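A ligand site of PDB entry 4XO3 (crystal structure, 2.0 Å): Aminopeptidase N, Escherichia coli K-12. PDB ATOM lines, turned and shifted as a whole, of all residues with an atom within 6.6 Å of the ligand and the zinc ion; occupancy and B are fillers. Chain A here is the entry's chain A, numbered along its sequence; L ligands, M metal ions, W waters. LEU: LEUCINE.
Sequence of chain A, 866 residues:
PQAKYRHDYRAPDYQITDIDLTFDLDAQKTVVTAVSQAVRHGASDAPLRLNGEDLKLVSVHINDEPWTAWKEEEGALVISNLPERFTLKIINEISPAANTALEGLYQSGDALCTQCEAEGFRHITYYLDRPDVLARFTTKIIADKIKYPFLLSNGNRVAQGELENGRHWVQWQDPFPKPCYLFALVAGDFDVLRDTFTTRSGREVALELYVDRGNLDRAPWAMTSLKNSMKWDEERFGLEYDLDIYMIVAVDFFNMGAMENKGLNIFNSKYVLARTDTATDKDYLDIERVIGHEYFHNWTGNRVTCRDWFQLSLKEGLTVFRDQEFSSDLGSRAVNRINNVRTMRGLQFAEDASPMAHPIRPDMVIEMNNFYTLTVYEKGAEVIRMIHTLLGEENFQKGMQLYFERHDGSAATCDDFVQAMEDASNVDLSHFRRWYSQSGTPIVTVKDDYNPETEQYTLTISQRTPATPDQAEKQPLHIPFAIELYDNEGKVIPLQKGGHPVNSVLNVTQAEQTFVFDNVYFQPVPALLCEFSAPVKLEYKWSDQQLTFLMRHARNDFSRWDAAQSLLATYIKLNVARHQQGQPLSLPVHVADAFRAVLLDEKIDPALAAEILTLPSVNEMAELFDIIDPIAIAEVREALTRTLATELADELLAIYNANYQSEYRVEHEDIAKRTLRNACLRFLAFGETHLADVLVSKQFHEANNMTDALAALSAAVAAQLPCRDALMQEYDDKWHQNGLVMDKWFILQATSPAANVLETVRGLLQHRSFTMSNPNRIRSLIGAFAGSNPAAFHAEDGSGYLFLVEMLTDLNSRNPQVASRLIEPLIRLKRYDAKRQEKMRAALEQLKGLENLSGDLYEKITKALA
The side-chain carboxylate (OE1) of Glu 260 is in salt-bridge range of a nitrogen (N) of the ligand, 2.7 Å away.
SD of Met 259 sits at hydrogen-bond distance from N of the ligand (3.7 Å).
OE1 of Glu 117 lies within salt-bridge range of N of the ligand, at 2.5 Å.
An oxygen (OXT) of the ligand lies within hydrogen-bond range of the side-chain hydroxyl of Tyr 377 (2.7 Å).
OE1 of Glu 316 sits close to OH of Tyr 377 (3.5 Å).
The side-chain amide nitrogen of Gln 115 lies within hydrogen-bond range of the backbone carbonyl oxygen of Glu 117 (3.0 Å).
The backbone NH (N) of Glu 260 lies within hydrogen-bond range of the side-chain carboxylate (OE1) of Glu 294, 3.4 Å away.
ND1 of His 297 sits at hydrogen-bond distance from OG1 of Thr 319, at 3.2 Å.
The side-chain amino group (NZ) of Lys 315 is in salt-bridge range of the side-chain carboxylate (OE2) of Glu 316 (2.8 Å).
SD of Met 256 sits close to NH1 of Arg 821.
NE2 of Gln 115 sits at hydrogen-bond distance from SD of Met 259, at 3.6 Å.
The side-chain amino group (NZ) of Lys 315 lies within salt-bridge range of the side-chain carboxylate (OE2) of Glu 117 (2.7 Å).
OE1 of Glu 294 sits close to O of the ligand (3.3 Å).
Residues that only touch the ligand: Ala 258 (3.4 Å), Lys 315 (3.6 Å), Met 256 (3.7 Å), Gln 115 (3.7 Å) and Tyr 372 (3.7 Å).
Hydrophobic or aromatic side chains within 4 Å of the ligand: Met 256, Met 259, His 293, His 297, Tyr 372 and Tyr 377.
13 residues have an atom within 4 Å of the ligand: Gln 115, Glu 117, Met 256, Ala 258, Met 259, Glu 260, His 293, Glu 294, His 297, Lys 315, Glu 316, Tyr 372 and Tyr 377.
The nearest printed residue that does not touch the ligand is Phe 254 (4.4 Å).
The zinc ion is bound by the side-chain carboxylate (OE1) of Glu 316.
The zinc ion is bound by a ring nitrogen (NE2) of His 293.
O of the ligand is bound to the zinc ion, at 2.0 Å.
The zinc ion is bound by NE2 of His 297.
The zinc ion has four donor atoms within binding distance.
Water W2 lies within hydrogen-bond range of N of Gly 257 (2.9 Å), OXT of the ligand (3.0 Å) and N of Ala 258 (3.1 Å).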
ATOM      1  N   GLN A 115       5.692  22.434 -34.401  1.00  0.00           N
ATOM      2  CA  GLN A 115       5.731  23.414 -33.282  1.00  0.00           C
ATOM      3  C   GLN A 115       4.821  24.543 -33.729  1.00  0.00           C
ATOM      4  O   GLN A 115       5.106  25.238 -34.730  1.00  0.00           O
ATOM      5  CB  GLN A 115       7.153  23.906 -32.931  1.00  0.00           C
ATOM      6  CG  GLN A 115       7.135  25.048 -31.923  1.00  0.00           C
ATOM      7  CD  GLN A 115       6.423  24.643 -30.623  1.00  0.00           C
ATOM      8  OE1 GLN A 115       6.486  23.505 -30.190  1.00  0.00           O
ATOM      9  NE2 GLN A 115       5.776  25.604 -29.980  1.00  0.00           N
ATOM     10  N   GLU A 117       3.108  26.850 -31.294  1.00  0.00           N
ATOM     11  CA  GLU A 117       3.113  28.060 -30.446  1.00  0.00           C
ATOM     12  C   GLU A 117       4.307  28.958 -30.850  1.00  0.00           C
ATOM     13  O   GLU A 117       5.415  28.431 -30.982  1.00  0.00           O
ATOM     14  CB  GLU A 117       3.185  27.708 -28.952  1.00  0.00           C
ATOM     15  CG  GLU A 117       2.882  28.918 -28.081  1.00  0.00           C
ATOM     16  CD  GLU A 117       2.955  28.703 -26.585  1.00  0.00           C
ATOM     17  OE1 GLU A 117       3.142  27.549 -26.170  1.00  0.00           O
ATOM     18  OE2 GLU A 117       2.739  29.712 -25.870  1.00  0.00           O
ATOM     19  N   ALA A 118       4.118  30.275 -31.025  1.00  0.00           N
ATOM     20  CA  ALA A 118       2.837  30.997 -30.867  1.00  0.00           C
ATOM     21  C   ALA A 118       1.975  30.992 -32.119  1.00  0.00           C
ATOM     22  O   ALA A 118       0.730  30.826 -31.996  1.00  0.00           O
ATOM     23  CB  ALA A 118       3.136  32.466 -30.529  1.00  0.00           C
ATOM     24  N   TYR A 181      -2.634  26.776 -31.474  1.00  0.00           N
ATOM     25  CA  TYR A 181      -1.237  26.657 -30.997  1.00  0.00           C
ATOM     26  C   TYR A 181      -1.004  25.347 -30.253  1.00  0.00           C
ATOM     27  O   TYR A 181       0.154  24.957 -30.091  1.00  0.00           O
ATOM     28  CB  TYR A 181      -0.710  27.833 -30.180  1.00  0.00           C
ATOM     29  CG  TYR A 181      -1.169  27.883 -28.706  1.00  0.00           C
ATOM     30  CD1 TYR A 181      -0.428  27.250 -27.698  1.00  0.00           C
ATOM     31  CD2 TYR A 181      -2.357  28.594 -28.310  1.00  0.00           C
ATOM     32  CE1 TYR A 181      -0.834  27.301 -26.373  1.00  0.00           C
ATOM     33  CE2 TYR A 181      -2.750  28.611 -26.987  1.00  0.00           C
ATOM     34  CZ  TYR A 181      -1.997  27.946 -26.017  1.00  0.00           C
ATOM     35  OH  TYR A 181      -2.385  27.962 -24.718  1.00  0.00           O
ATOM     36  N   PHE A 254      14.676  21.283 -31.865  1.00  0.00           N
ATOM     37  CA  PHE A 254      13.594  22.002 -31.197  1.00  0.00           C
ATOM     38  C   PHE A 254      14.177  23.331 -30.746  1.00  0.00           C
ATOM     39  O   PHE A 254      15.209  23.368 -30.085  1.00  0.00           O
ATOM     40  CB  PHE A 254      13.083  21.186 -30.004  1.00  0.00           C
ATOM     41  CG  PHE A 254      11.735  21.586 -29.518  1.00  0.00           C
ATOM     42  CD1 PHE A 254      10.573  21.282 -30.292  1.00  0.00           C
ATOM     43  CD2 PHE A 254      11.587  22.329 -28.335  1.00  0.00           C
ATOM     44  CE1 PHE A 254       9.344  21.656 -29.853  1.00  0.00           C
ATOM     45  CE2 PHE A 254      10.331  22.741 -27.934  1.00  0.00           C
ATOM     46  CZ  PHE A 254       9.204  22.409 -28.702  1.00  0.00           C
ATOM     47  N   MET A 256      12.963  25.524 -28.517  1.00  0.00           N
ATOM     48  CA  MET A 256      12.758  25.901 -27.099  1.00  0.00           C
ATOM     49  C   MET A 256      12.992  24.678 -26.208  1.00  0.00           C
ATOM     50  O   MET A 256      13.857  23.832 -26.486  1.00  0.00           O
ATOM     51  CB  MET A 256      11.332  26.491 -27.001  1.00  0.00           C
ATOM     52  CG  MET A 256      11.107  27.729 -27.878  1.00  0.00           C
ATOM     53  SD  MET A 256      11.840  29.062 -26.922  1.00  0.00           S
ATOM     54  CE  MET A 256      10.733  29.289 -25.452  1.00  0.00           C
ATOM     55  N   GLY A 257      12.270  24.580 -25.110  1.00  0.00           N
ATOM     56  CA  GLY A 257      12.448  23.520 -24.149  1.00  0.00           C
ATOM     57  C   GLY A 257      11.465  22.386 -24.406  1.00  0.00           C
ATOM     58  O   GLY A 257      11.840  21.246 -24.582  1.00  0.00           O
ATOM     59  N   ALA A 258      10.204  22.685 -24.267  1.00  0.00           N
ATOM     60  CA  ALA A 258       9.173  21.683 -24.505  1.00  0.00           C
ATOM     61  C   ALA A 258       7.827  22.352 -24.685  1.00  0.00           C
ATOM     62  O   ALA A 258       7.657  23.548 -24.397  1.00  0.00           O
ATOM     63  CB  ALA A 258       9.115  20.673 -23.375  1.00  0.00           C
ATOM     64  N   MET A 259       6.827  21.572 -25.106  1.00  0.00           N
ATOM     65  CA  MET A 259       5.545  22.139 -25.534  1.00  0.00           C
ATOM     66  C   MET A 259       4.356  21.299 -25.110  1.00  0.00           C
ATOM     67  O   MET A 259       4.336  20.058 -25.311  1.00  0.00           O
ATOM     68  CB  MET A 259       5.544  22.333 -27.006  1.00  0.00           C
ATOM     69  CG  MET A 259       4.230  22.827 -27.590  1.00  0.00           C
ATOM     70  SD  MET A 259       4.021  24.573 -27.040  1.00  0.00           S
ATOM     71  CE  MET A 259       2.232  24.635 -27.022  1.00  0.00           C
ATOM     72  N   GLU A 260       3.410  21.983 -24.519  1.00  0.00           N
ATOM     73  CA  GLU A 260       2.222  21.366 -23.811  1.00  0.00           C
ATOM     74  C   GLU A 260       1.055  20.934 -24.728  1.00  0.00           C
ATOM     75  O   GLU A 260      -0.126  20.936 -24.297  1.00  0.00           O
ATOM     76  CB  GLU A 260       1.714  22.262 -22.712  1.00  0.00           C
ATOM     77  CG  GLU A 260       0.998  23.572 -23.171  1.00  0.00           C
ATOM     78  CD  GLU A 260       1.973  24.758 -23.330  1.00  0.00           C
ATOM     79  OE1 GLU A 260       3.224  24.594 -23.502  1.00  0.00           O
ATOM     80  OE2 GLU A 260       1.440  25.915 -23.344  1.00  0.00           O
ATOM     81  N   HIS A 293       6.315  21.038 -15.715  1.00  0.00           N
ATOM     82  CA  HIS A 293       5.835  22.281 -16.330  1.00  0.00           C
ATOM     83  C   HIS A 293       4.824  21.995 -17.416  1.00  0.00           C
ATOM     84  O   HIS A 293       3.713  22.536 -17.380  1.00  0.00           O
ATOM     85  CB  HIS A 293       7.051  23.097 -16.873  1.00  0.00           C
ATOM     86  CG  HIS A 293       6.715  24.408 -17.480  1.00  0.00           C
ATOM     87  ND1 HIS A 293       6.791  25.596 -16.790  1.00  0.00           N
ATOM     88  CD2 HIS A 293       6.266  24.727 -18.718  1.00  0.00           C
ATOM     89  CE1 HIS A 293       6.301  26.568 -17.533  1.00  0.00           C
ATOM     90  NE2 HIS A 293       6.029  26.078 -18.719  1.00  0.00           N
ATOM     91  N   GLU A 294       5.206  21.209 -18.417  1.00  0.00           N
ATOM     92  CA  GLU A 294       4.288  20.923 -19.530  1.00  0.00           C
ATOM     93  C   GLU A 294       3.025  20.211 -19.071  1.00  0.00           C
ATOM     94  O   GLU A 294       1.947  20.501 -19.532  1.00  0.00           O
ATOM     95  CB  GLU A 294       4.989  20.226 -20.654  1.00  0.00           C
ATOM     96  CG  GLU A 294       6.315  20.884 -21.090  1.00  0.00           C
ATOM     97  CD  GLU A 294       6.274  22.338 -21.441  1.00  0.00           C
ATOM     98  OE1 GLU A 294       5.214  22.830 -21.763  1.00  0.00           O
ATOM     99  OE2 GLU A 294       7.344  22.979 -21.366  1.00  0.00           O
ATOM    100  N   HIS A 297       0.605  22.678 -17.509  1.00  0.00           N
ATOM    101  CA  HIS A 297      -0.089  23.471 -18.447  1.00  0.00           C
ATOM    102  C   HIS A 297      -1.450  22.825 -18.839  1.00  0.00           C
ATOM    103  O   HIS A 297      -2.339  23.466 -19.420  1.00  0.00           O
ATOM    104  CB  HIS A 297       0.722  23.602 -19.718  1.00  0.00           C
ATOM    105  CG  HIS A 297       1.614  24.803 -19.800  1.00  0.00           C
ATOM    106  ND1 HIS A 297       1.161  26.084 -19.586  1.00  0.00           N
ATOM    107  CD2 HIS A 297       2.934  24.911 -20.117  1.00  0.00           C
ATOM    108  CE1 HIS A 297       2.175  26.935 -19.731  1.00  0.00           C
ATOM    109  NE2 HIS A 297       3.235  26.246 -20.077  1.00  0.00           N
ATOM    110  N   LEU A 312       0.186  36.052 -22.332  1.00  0.00           N
ATOM    111  CA  LEU A 312       1.021  34.877 -22.243  1.00  0.00           C
ATOM    112  C   LEU A 312       1.378  34.514 -20.787  1.00  0.00           C
ATOM    113  O   LEU A 312       1.363  33.327 -20.415  1.00  0.00           O
ATOM    114  CB  LEU A 312       2.308  35.050 -23.033  1.00  0.00           C
ATOM    115  CG  LEU A 312       3.300  33.901 -23.052  1.00  0.00           C
ATOM    116  CD1 LEU A 312       2.657  32.601 -23.583  1.00  0.00           C
ATOM    117  CD2 LEU A 312       4.523  34.236 -23.905  1.00  0.00           C
ATOM    118  N   LYS A 315      -0.636  31.969 -18.508  1.00  0.00           N
ATOM    119  CA  LYS A 315      -0.277  30.572 -18.465  1.00  0.00           C
ATOM    120  C   LYS A 315       1.198  30.409 -18.083  1.00  0.00           C
ATOM    121  O   LYS A 315       1.522  29.457 -17.337  1.00  0.00           O
ATOM    122  CB  LYS A 315      -0.634  29.824 -19.750  1.00  0.00           C
ATOM    123  CG  LYS A 315       0.137  30.159 -21.028  1.00  0.00           C
ATOM    124  CD  LYS A 315      -0.399  29.309 -22.197  1.00  0.00           C
ATOM    125  CE  LYS A 315       0.375  29.468 -23.475  1.00  0.00           C
ATOM    126  NZ  LYS A 315       1.680  28.804 -23.590  1.00  0.00           N
ATOM    127  N   GLU A 316       2.103  31.290 -18.564  1.00  0.00           N
ATOM    128  CA  GLU A 316       3.546  30.983 -18.323  1.00  0.00           C
ATOM    129  C   GLU A 316       3.977  31.301 -16.897  1.00  0.00           C
ATOM    130  O   GLU A 316       4.686  30.504 -16.299  1.00  0.00           O
ATOM    131  CB  GLU A 316       4.522  31.526 -19.364  1.00  0.00           C
ATOM    132  CG  GLU A 316       4.239  31.012 -20.754  1.00  0.00           C
ATOM    133  CD  GLU A 316       4.333  29.511 -20.861  1.00  0.00           C
ATOM    134  OE1 GLU A 316       5.016  28.890 -19.982  1.00  0.00           O
ATOM    135  OE2 GLU A 316       3.873  29.009 -21.912  1.00  0.00           O
ATOM    136  N   THR A 319       2.301  28.694 -14.659  1.00  0.00           N
ATOM    137  CA  THR A 319       2.837  27.372 -14.810  1.00  0.00           C
ATOM    138  C   THR A 319       4.285  27.273 -14.289  1.00  0.00           C
ATOM    139  O   THR A 319       4.670  26.237 -13.743  1.00  0.00           O
ATOM    140  CB  THR A 319       2.688  26.894 -16.231  1.00  0.00           C
ATOM    141  OG1 THR A 319       1.291  26.920 -16.545  1.00  0.00           O
ATOM    142  CG2 THR A 319       3.195  25.472 -16.421  1.00  0.00           C
ATOM    143  N   VAL A 320       5.076  28.330 -14.448  1.00  0.00           N
ATOM    144  CA  VAL A 320       6.390  28.380 -13.806  1.00  0.00           C
ATOM    145  C   VAL A 320       6.249  28.312 -12.298  1.00  0.00           C
ATOM    146  O   VAL A 320       6.965  27.579 -11.634  1.00  0.00           O
ATOM    147  CB  VAL A 320       7.187  29.636 -14.218  1.00  0.00           C
ATOM    148  CG1 VAL A 320       8.458  29.747 -13.348  1.00  0.00           C
ATOM    149  CG2 VAL A 320       7.548  29.540 -15.668  1.00  0.00           C
ATOM    150  N   ASN A 369       7.205  35.667 -30.844  1.00  0.00           N
ATOM    151  CA  ASN A 369       8.165  34.691 -30.360  1.00  0.00           C
ATOM    152  C   ASN A 369       9.301  35.368 -29.615  1.00  0.00           C
ATOM    153  O   ASN A 369      10.037  34.663 -28.887  1.00  0.00           O
ATOM    154  CB  ASN A 369       8.687  33.707 -31.422  1.00  0.00           C
ATOM    155  CG  ASN A 369       7.566  32.771 -31.960  1.00  0.00           C
ATOM    156  OD1 ASN A 369       7.291  32.718 -33.162  1.00  0.00           O
ATOM    157  ND2 ASN A 369       6.901  32.170 -31.110  1.00  0.00           N
ATOM    158  N   TYR A 372       8.808  35.272 -25.210  1.00  0.00           N
ATOM    159  CA  TYR A 372       8.924  34.070 -24.380  1.00  0.00           C
ATOM    160  C   TYR A 372      10.134  34.299 -23.481  1.00  0.00           C
ATOM    161  O   TYR A 372      11.187  33.681 -23.656  1.00  0.00           O
ATOM    162  CB  TYR A 372       8.994  32.805 -25.277  1.00  0.00           C
ATOM    163  CG  TYR A 372       7.607  32.509 -25.792  1.00  0.00           C
ATOM    164  CD1 TYR A 372       7.070  33.202 -26.862  1.00  0.00           C
ATOM    165  CD2 TYR A 372       6.826  31.550 -25.200  1.00  0.00           C
ATOM    166  CE1 TYR A 372       5.739  33.062 -27.219  1.00  0.00           C
ATOM    167  CE2 TYR A 372       5.515  31.334 -25.590  1.00  0.00           C
ATOM    168  CZ  TYR A 372       4.987  32.053 -26.667  1.00  0.00           C
ATOM    169  OH  TYR A 372       3.682  31.901 -27.028  1.00  0.00           O
ATOM    170  N   TYR A 377       8.080  34.686 -17.992  1.00  0.00           N
ATOM    171  CA  TYR A 377       8.147  33.417 -17.295  1.00  0.00           C
ATOM    172  C   TYR A 377       8.517  33.612 -15.793  1.00  0.00           C
ATOM    173  O   TYR A 377       7.703  33.332 -14.895  1.00  0.00           O
ATOM    174  CB  TYR A 377       9.147  32.522 -17.947  1.00  0.00           C
ATOM    175  CG  TYR A 377       8.646  31.794 -19.130  1.00  0.00           C
ATOM    176  CD1 TYR A 377       8.308  32.452 -20.292  1.00  0.00           C
ATOM    177  CD2 TYR A 377       8.539  30.398 -19.097  1.00  0.00           C
ATOM    178  CE1 TYR A 377       7.849  31.772 -21.425  1.00  0.00           C
ATOM    179  CE2 TYR A 377       8.130  29.711 -20.226  1.00  0.00           C
ATOM    180  CZ  TYR A 377       7.764  30.376 -21.393  1.00  0.00           C
ATOM    181  OH  TYR A 377       7.320  29.691 -22.486  1.00  0.00           O
ATOM    182  N   ARG A 821      17.297  34.819 -29.943  1.00  0.00           N
ATOM    183  CA  ARG A 821      17.848  34.484 -28.624  1.00  0.00           C
ATOM    184  C   ARG A 821      19.338  34.818 -28.506  1.00  0.00           C
ATOM    185  O   ARG A 821      19.770  35.383 -27.499  1.00  0.00           O
ATOM    186  CB  ARG A 821      17.668  32.954 -28.322  1.00  0.00           C
ATOM    187  CG  ARG A 821      16.239  32.502 -28.187  1.00  0.00           C
ATOM    188  CD  ARG A 821      15.684  32.844 -26.818  1.00  0.00           C
ATOM    189  NE  ARG A 821      14.353  32.257 -26.653  1.00  0.00           N
ATOM    190  CZ  ARG A 821      13.407  32.654 -25.762  1.00  0.00           C
ATOM    191  NH1 ARG A 821      12.238  32.062 -25.733  1.00  0.00           N
ATOM    192  NH2 ARG A 821      13.640  33.574 -24.889  1.00  0.00           N
HETATM  193  N   LEU L   1       4.571  26.820 -24.199  1.00  0.00           N
HETATM  194  CA  LEU L   1       6.033  26.499 -24.194  1.00  0.00           C
HETATM  195  C   LEU L   1       6.517  26.551 -22.767  1.00  0.00           C
HETATM  196  O   LEU L   1       5.813  26.063 -21.896  1.00  0.00           O
HETATM  197  CB  LEU L   1       6.806  27.490 -25.054  1.00  0.00           C
HETATM  198  CG  LEU L   1       6.725  27.222 -26.588  1.00  0.00           C
HETATM  199  CD1 LEU L   1       7.054  28.488 -27.394  1.00  0.00           C
HETATM  200  CD2 LEU L   1       7.700  26.077 -26.904  1.00  0.00           C
HETATM  201  OXT LEU L   1       7.629  27.057 -22.451  1.00  0.00           O
HETATM  202 ZN    ZN M   1       5.121  26.969 -20.235  1.00  0.00          ZN
HETATM  203  O   HOH W   1       8.069  30.910 -28.977  1.00  0.00           O
HETATM  204  O   HOH W   2      10.024  25.751 -23.668  1.00  0.00           O
